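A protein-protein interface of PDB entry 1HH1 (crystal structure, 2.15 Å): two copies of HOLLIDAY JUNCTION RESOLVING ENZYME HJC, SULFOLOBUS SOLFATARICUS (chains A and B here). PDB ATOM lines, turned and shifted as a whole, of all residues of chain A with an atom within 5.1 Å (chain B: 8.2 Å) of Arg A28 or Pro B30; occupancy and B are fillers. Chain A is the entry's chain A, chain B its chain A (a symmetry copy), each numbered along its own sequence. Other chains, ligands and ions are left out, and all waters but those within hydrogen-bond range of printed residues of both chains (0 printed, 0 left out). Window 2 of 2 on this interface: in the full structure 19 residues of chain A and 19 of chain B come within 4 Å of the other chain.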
ATOM      1  N   SER A   9     -14.402  -5.127   8.751  1.00  0.00           N
ATOM      2  CA  SER A   9     -13.027  -5.445   9.250  1.00  0.00           C
ATOM      3  C   SER A   9     -12.952  -6.946   9.515  1.00  0.00           C
ATOM      4  O   SER A   9     -12.074  -7.629   8.996  1.00  0.00           O
ATOM      5  CB  SER A   9     -12.673  -4.647  10.490  1.00  0.00           C
ATOM      6  OG  SER A   9     -11.329  -4.188  10.465  1.00  0.00           O
ATOM      7  N   GLU A  12     -13.450  -8.376   6.139  1.00  0.00           N
ATOM      8  CA  GLU A  12     -12.299  -8.128   5.287  1.00  0.00           C
ATOM      9  C   GLU A  12     -11.206  -9.157   5.558  1.00  0.00           C
ATOM     10  O   GLU A  12     -10.706  -9.829   4.656  1.00  0.00           O
ATOM     11  CB  GLU A  12     -11.732  -6.720   5.474  1.00  0.00           C
ATOM     12  CG  GLU A  12     -12.522  -5.659   4.739  1.00  0.00           C
ATOM     13  CD  GLU A  12     -11.933  -4.268   4.784  1.00  0.00           C
ATOM     14  OE1 GLU A  12     -10.702  -4.111   4.900  1.00  0.00           O
ATOM     15  OE2 GLU A  12     -12.710  -3.297   4.669  1.00  0.00           O
ATOM     16  N   ARG A  13     -10.887  -9.277   6.841  1.00  0.00           N
ATOM     17  CA  ARG A  13      -9.898 -10.218   7.343  1.00  0.00           C
ATOM     18  C   ARG A  13     -10.199 -11.654   6.955  1.00  0.00           C
ATOM     19  O   ARG A  13      -9.296 -12.353   6.495  1.00  0.00           O
ATOM     20  CB  ARG A  13      -9.728 -10.091   8.868  1.00  0.00           C
ATOM     21  CG  ARG A  13      -9.125  -8.758   9.261  1.00  0.00           C
ATOM     22  CD  ARG A  13      -8.694  -8.633  10.706  1.00  0.00           C
ATOM     23  NE  ARG A  13      -7.980  -7.396  11.022  1.00  0.00           N
ATOM     24  CZ  ARG A  13      -8.394  -6.145  10.858  1.00  0.00           C
ATOM     25  NH1 ARG A  13      -9.580  -5.891  10.317  1.00  0.00           N
ATOM     26  NH2 ARG A  13      -7.639  -5.105  11.203  1.00  0.00           N
ATOM     27  N   VAL A  16      -9.526 -11.844   3.131  1.00  0.00           N
ATOM     28  CA  VAL A  16      -8.087 -11.854   2.809  1.00  0.00           C
ATOM     29  C   VAL A  16      -7.491 -13.229   3.030  1.00  0.00           C
ATOM     30  O   VAL A  16      -6.750 -13.789   2.223  1.00  0.00           O
ATOM     31  CB  VAL A  16      -7.411 -10.749   3.642  1.00  0.00           C
ATOM     32  CG1 VAL A  16      -5.907 -10.874   3.712  1.00  0.00           C
ATOM     33  CG2 VAL A  16      -7.779  -9.401   2.966  1.00  0.00           C
ATOM     34  N   VAL A  26      -2.130 -11.022  -1.351  1.00  0.00           N
ATOM     35  CA  VAL A  26      -3.115 -10.012  -1.000  1.00  0.00           C
ATOM     36  C   VAL A  26      -2.567  -8.901  -0.134  1.00  0.00           C
ATOM     37  O   VAL A  26      -1.791  -9.156   0.798  1.00  0.00           O
ATOM     38  CB  VAL A  26      -4.272 -10.716  -0.214  1.00  0.00           C
ATOM     39  CG1 VAL A  26      -5.396  -9.740   0.119  1.00  0.00           C
ATOM     40  CG2 VAL A  26      -4.893 -11.905  -0.951  1.00  0.00           C
ATOM     41  N   VAL A  27      -3.013  -7.676  -0.390  1.00  0.00           N
ATOM     42  CA  VAL A  27      -2.685  -6.546   0.461  1.00  0.00           C
ATOM     43  C   VAL A  27      -3.935  -5.730   0.772  1.00  0.00           C
ATOM     44  O   VAL A  27      -4.860  -5.551  -0.025  1.00  0.00           O
ATOM     45  CB  VAL A  27      -1.561  -5.669  -0.112  1.00  0.00           C
ATOM     46  CG1 VAL A  27      -1.911  -5.042  -1.447  1.00  0.00           C
ATOM     47  CG2 VAL A  27      -1.162  -4.577   0.867  1.00  0.00           C
ATOM     48  N   ARG A  28      -4.049  -5.289   2.010  1.00  0.00           N
ATOM     49  CA  ARG A  28      -5.184  -4.448   2.411  1.00  0.00           C
ATOM     50  C   ARG A  28      -4.785  -2.995   2.264  1.00  0.00           C
ATOM     51  O   ARG A  28      -3.603  -2.708   2.444  1.00  0.00           O
ATOM     52  CB  ARG A  28      -5.583  -4.777   3.845  1.00  0.00           C
ATOM     53  CG  ARG A  28      -6.291  -6.136   3.854  1.00  0.00           C
ATOM     54  CD  ARG A  28      -6.590  -6.600   5.274  1.00  0.00           C
ATOM     55  NE  ARG A  28      -7.791  -5.945   5.768  1.00  0.00           N
ATOM     56  CZ  ARG A  28      -8.177  -5.903   7.040  1.00  0.00           C
ATOM     57  NH1 ARG A  28      -7.426  -6.498   7.957  1.00  0.00           N
ATOM     58  NH2 ARG A  28      -9.298  -5.265   7.356  1.00  0.00           N
ATOM     59  N   ALA A  29      -5.632  -2.139   1.723  1.00  0.00           N
ATOM     60  CA  ALA A  29      -5.261  -0.727   1.638  1.00  0.00           C
ATOM     61  C   ALA A  29      -5.033  -0.236   3.072  1.00  0.00           C
ATOM     62  O   ALA A  29      -5.808  -0.544   3.960  1.00  0.00           O
ATOM     63  CB  ALA A  29      -6.369   0.074   0.984  1.00  0.00           C
ATOM     64  N   PRO A  30      -3.950   0.472   3.291  1.00  0.00           N
ATOM     65  CA  PRO A  30      -3.598   1.069   4.571  1.00  0.00           C
ATOM     66  C   PRO A  30      -4.652   2.113   4.924  1.00  0.00           C
ATOM     67  O   PRO A  30      -5.231   2.708   4.009  1.00  0.00           O
ATOM     68  CB  PRO A  30      -2.205   1.699   4.429  1.00  0.00           C
ATOM     69  CG  PRO A  30      -1.790   1.305   3.033  1.00  0.00           C
ATOM     70  CD  PRO A  30      -2.996   0.855   2.235  1.00  0.00           C
ATOM     71  N   ASP A  42     -10.342  -1.606  -0.930  1.00  0.00           N
ATOM     72  CA  ASP A  42     -10.009  -2.193   0.375  1.00  0.00           C
ATOM     73  C   ASP A  42      -9.046  -3.373   0.227  1.00  0.00           C
ATOM     74  O   ASP A  42      -8.186  -3.626   1.056  1.00  0.00           O
ATOM     75  CB  ASP A  42     -11.268  -2.704   1.095  1.00  0.00           C
ATOM     76  CG  ASP A  42     -12.210  -1.556   1.463  1.00  0.00           C
ATOM     77  OD1 ASP A  42     -11.760  -0.516   1.958  1.00  0.00           O
ATOM     78  OD2 ASP A  42     -13.414  -1.635   1.211  1.00  0.00           O
ATOM     79  N   ILE A  43      -9.359  -4.240  -0.739  1.00  0.00           N
ATOM     80  CA  ILE A  43      -8.608  -5.473  -0.916  1.00  0.00           C
ATOM     81  C   ILE A  43      -8.002  -5.512  -2.307  1.00  0.00           C
ATOM     82  O   ILE A  43      -8.677  -5.363  -3.333  1.00  0.00           O
ATOM     83  CB  ILE A  43      -9.484  -6.711  -0.617  1.00  0.00           C
ATOM     84  CG1 ILE A  43     -10.046  -6.725   0.828  1.00  0.00           C
ATOM     85  CG2 ILE A  43      -8.662  -7.997  -0.803  1.00  0.00           C
ATOM     86  CD1 ILE A  43     -11.051  -7.867   1.038  1.00  0.00           C
ATOM     87  N   VAL B  27       0.069   0.891  -4.040  1.00  0.00           N
ATOM     88  CA  VAL B  27      -0.264   0.724  -2.636  1.00  0.00           C
ATOM     89  C   VAL B  27       0.984   0.386  -1.827  1.00  0.00           C
ATOM     90  O   VAL B  27       1.911  -0.312  -2.246  1.00  0.00           O
ATOM     91  CB  VAL B  27      -1.387  -0.298  -2.404  1.00  0.00           C
ATOM     92  CG1 VAL B  27      -1.033  -1.695  -2.873  1.00  0.00           C
ATOM     93  CG2 VAL B  27      -1.791  -0.348  -0.939  1.00  0.00           C
ATOM     94  N   ARG B  28       1.093   0.975  -0.652  1.00  0.00           N
ATOM     95  CA  ARG B  28       2.225   0.684   0.237  1.00  0.00           C
ATOM     96  C   ARG B  28       1.824  -0.428   1.183  1.00  0.00           C
ATOM     97  O   ARG B  28       0.641  -0.498   1.510  1.00  0.00           O
ATOM     98  CB  ARG B  28       2.619   1.948   0.993  1.00  0.00           C
ATOM     99  CG  ARG B  28       3.330   2.896   0.021  1.00  0.00           C
ATOM    100  CD  ARG B  28       3.624   4.242   0.669  1.00  0.00           C
ATOM    101  NE  ARG B  28       4.822   4.148   1.488  1.00  0.00           N
ATOM    102  CZ  ARG B  28       5.203   5.038   2.400  1.00  0.00           C
ATOM    103  NH1 ARG B  28       4.450   6.111   2.603  1.00  0.00           N
ATOM    104  NH2 ARG B  28       6.322   4.827   3.084  1.00  0.00           N
ATOM    105  N   ALA B  29       2.671  -1.409   1.430  1.00  0.00           N
ATOM    106  CA  ALA B  29       2.299  -2.448   2.389  1.00  0.00           C
ATOM    107  C   ALA B  29       2.065  -1.752   3.735  1.00  0.00           C
ATOM    108  O   ALA B  29       2.837  -0.898   4.130  1.00  0.00           O
ATOM    109  CB  ALA B  29       3.408  -3.472   2.519  1.00  0.00           C
ATOM    110  N   PRO B  30       0.980  -2.086   4.394  1.00  0.00           N
ATOM    111  CA  PRO B  30       0.622  -1.576   5.709  1.00  0.00           C
ATOM    112  C   PRO B  30       1.674  -2.041   6.710  1.00  0.00           C
ATOM    113  O   PRO B  30       2.254  -3.113   6.510  1.00  0.00           O
ATOM    114  CB  PRO B  30      -0.771  -2.116   6.060  1.00  0.00           C
ATOM    115  CG  PRO B  30      -1.180  -2.852   4.808  1.00  0.00           C
ATOM    116  CD  PRO B  30       0.029  -3.116   3.936  1.00  0.00           C
ATOM    117  N   ALA B  31       1.946  -1.269   7.746  1.00  0.00           N
ATOM    118  CA  ALA B  31       2.955  -1.598   8.743  1.00  0.00           C
ATOM    119  C   ALA B  31       2.714  -2.864   9.547  1.00  0.00           C
ATOM    120  O   ALA B  31       1.600  -3.267   9.867  1.00  0.00           O
ATOM    121  CB  ALA B  31       3.128  -0.400   9.678  1.00  0.00           C
ATOM    122  N   PRO B  39       5.294 -11.268   4.961  1.00  0.00           N
ATOM    123  CA  PRO B  39       5.873  -9.996   4.571  1.00  0.00           C
ATOM    124  C   PRO B  39       5.638  -9.695   3.092  1.00  0.00           C
ATOM    125  O   PRO B  39       5.740 -10.504   2.188  1.00  0.00           O
ATOM    126  CB  PRO B  39       7.350  -9.937   4.926  1.00  0.00           C
ATOM    127  CG  PRO B  39       7.552 -11.266   5.620  1.00  0.00           C
ATOM    128  CD  PRO B  39       6.242 -11.942   5.866  1.00  0.00           C
ATOM    129  N   ILE B  40       5.211  -8.448   2.973  1.00  0.00           N
ATOM    130  CA  ILE B  40       4.754  -7.893   1.698  1.00  0.00           C
ATOM    131  C   ILE B  40       5.765  -6.889   1.194  1.00  0.00           C
ATOM    132  O   ILE B  40       6.362  -6.154   1.971  1.00  0.00           O
ATOM    133  CB  ILE B  40       3.395  -7.244   2.080  1.00  0.00           C
ATOM    134  CG1 ILE B  40       2.443  -8.382   2.525  1.00  0.00           C
ATOM    135  CG2 ILE B  40       2.763  -6.448   0.961  1.00  0.00           C
ATOM    136  CD1 ILE B  40       1.191  -7.878   3.202  1.00  0.00           C
ATOM    137  N   PRO B  41       5.991  -6.905  -0.104  1.00  0.00           N
ATOM    138  CA  PRO B  41       6.861  -5.940  -0.749  1.00  0.00           C
ATOM    139  C   PRO B  41       6.420  -4.564  -0.256  1.00  0.00           C
ATOM    140  O   PRO B  41       5.223  -4.295  -0.067  1.00  0.00           O
ATOM    141  CB  PRO B  41       6.713  -6.115  -2.263  1.00  0.00           C
ATOM    142  CG  PRO B  41       6.163  -7.534  -2.317  1.00  0.00           C
ATOM    143  CD  PRO B  41       5.365  -7.786  -1.075  1.00  0.00           C
ATOM    144  N   ASP B  42       7.390  -3.686  -0.004  1.00  0.00           N
ATOM    145  CA  ASP B  42       7.054  -2.338   0.474  1.00  0.00           C
ATOM    146  C   ASP B  42       6.093  -1.631  -0.483  1.00  0.00           C
ATOM    147  O   ASP B  42       5.231  -0.858  -0.095  1.00  0.00           O
ATOM    148  CB  ASP B  42       8.311  -1.463   0.609  1.00  0.00           C
ATOM    149  CG  ASP B  42       9.250  -1.990   1.695  1.00  0.00           C
ATOM    150  OD1 ASP B  42       8.796  -2.353   2.787  1.00  0.00           O
ATOM    151  OD2 ASP B  42      10.455  -2.115   1.468  1.00  0.00           O
ATOM    152  N   ILE B  44       3.759  -1.889  -4.008  1.00  0.00           N
ATOM    153  CA  ILE B  44       3.068  -2.687  -5.021  1.00  0.00           C
ATOM    154  C   ILE B  44       2.550  -1.692  -6.077  1.00  0.00           C
ATOM    155  O   ILE B  44       1.784  -0.763  -5.770  1.00  0.00           O
ATOM    156  CB  ILE B  44       1.936  -3.533  -4.425  1.00  0.00           C
ATOM    157  CG1 ILE B  44       2.555  -4.573  -3.491  1.00  0.00           C
ATOM    158  CG2 ILE B  44       1.076  -4.200  -5.497  1.00  0.00           C
ATOM    159  CD1 ILE B  44       1.762  -4.839  -2.255  1.00  0.00           C
ATOM    160  N   PHE B  79       5.512 -13.808  -2.218  1.00  0.00           N
ATOM    161  CA  PHE B  79       4.448 -12.873  -2.638  1.00  0.00           C
ATOM    162  C   PHE B  79       4.569 -12.625  -4.142  1.00  0.00           C
ATOM    163  O   PHE B  79       3.614 -12.674  -4.935  1.00  0.00           O
ATOM    164  CB  PHE B  79       4.522 -11.592  -1.810  1.00  0.00           C
ATOM    165  CG  PHE B  79       3.408 -10.624  -2.007  1.00  0.00           C
ATOM    166  CD1 PHE B  79       3.321  -9.880  -3.175  1.00  0.00           C
ATOM    167  CD2 PHE B  79       2.437 -10.455  -1.051  1.00  0.00           C
ATOM    168  CE1 PHE B  79       2.300  -8.974  -3.373  1.00  0.00           C
ATOM    169  CE2 PHE B  79       1.390  -9.554  -1.227  1.00  0.00           C
ATOM    170  CZ  PHE B  79       1.327  -8.815  -2.403  1.00  0.00           C
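Val B27 touches its own counterpart, Val A27.
Val A27 touches Pro B30, and with the chains exchanged Pro A30 touches Val B27.
Arg A28 touches Pro B30, and with the chains exchanged Pro A30 touches Arg B28.
Of the 7 pairs that touch across the chains among the printed residues, 5 have their exchanged pair printed and touching as well.
Val A27 touches just these residues of chain B: Val B27 (3.7 Å), Pro B30 (3.6 Å) and Ile B44 (3.8 Å).
Arg A28 touches just one residue of chain B: Pro B30 (3.4 Å).
No residue of chain B comes within 4 Å of Ala A29.
Of the printed residues of chain B, Pro A30 touches Val B27 (3.6 Å) and Arg B28 (3.4 Å).
Asp A42 touches none of the printed residues of chain B.
Of the printed residues of chain A, Val B27 touches Val A27 (3.7 Å) and Pro A30 (3.6 Å).
Printed residues of chain A within 4 Å of Arg B28: Pro A30.
Printed residues of chain A within 4 Å of Pro B30: Val A27 (3.6 Å) and Arg A28 (3.4 Å).
Printed residues of chain A within 4 Å of Ile B44: Val A27 (3.8 Å).
Of the printed residues of chain A, Phe B79 touches Val A26.
The nearest residue of chain B that does not touch Arg A28 is Val B27 (4.5 Å).
The nearest residue of chain A that does not touch Pro B30 is Pro A30 (4.4 Å).
The nearest printed residue of chain A that does not touch Arg B28 is Val A27 (4.5 Å).
The backbone carbonyl oxygen (O) of Ile B44 sits at hydrogen-bond distance from the backbone NH (N) of Val B27.
OE1 of Glu A12 is in salt-bridge range of NH2 of Arg A28 (3.1 Å).
Of the 11 printed residues of chain A, 4 touch a printed residue of chain B.
Hydrophobic or aromatic side chains of chain B within 4 Å of the printed part of chain A: Val B27, Pro B30, Ile B44 and Phe B79.
Among the printed residues, pairs that only touch across the chains: Val A26 with Phe B79, Val A27 with Val B27, Val A27 with Pro B30, Val A27 with Ile B44, Arg A28 with Pro B30, Pro A30 with Val B27 and Pro A30 with Arg B28.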
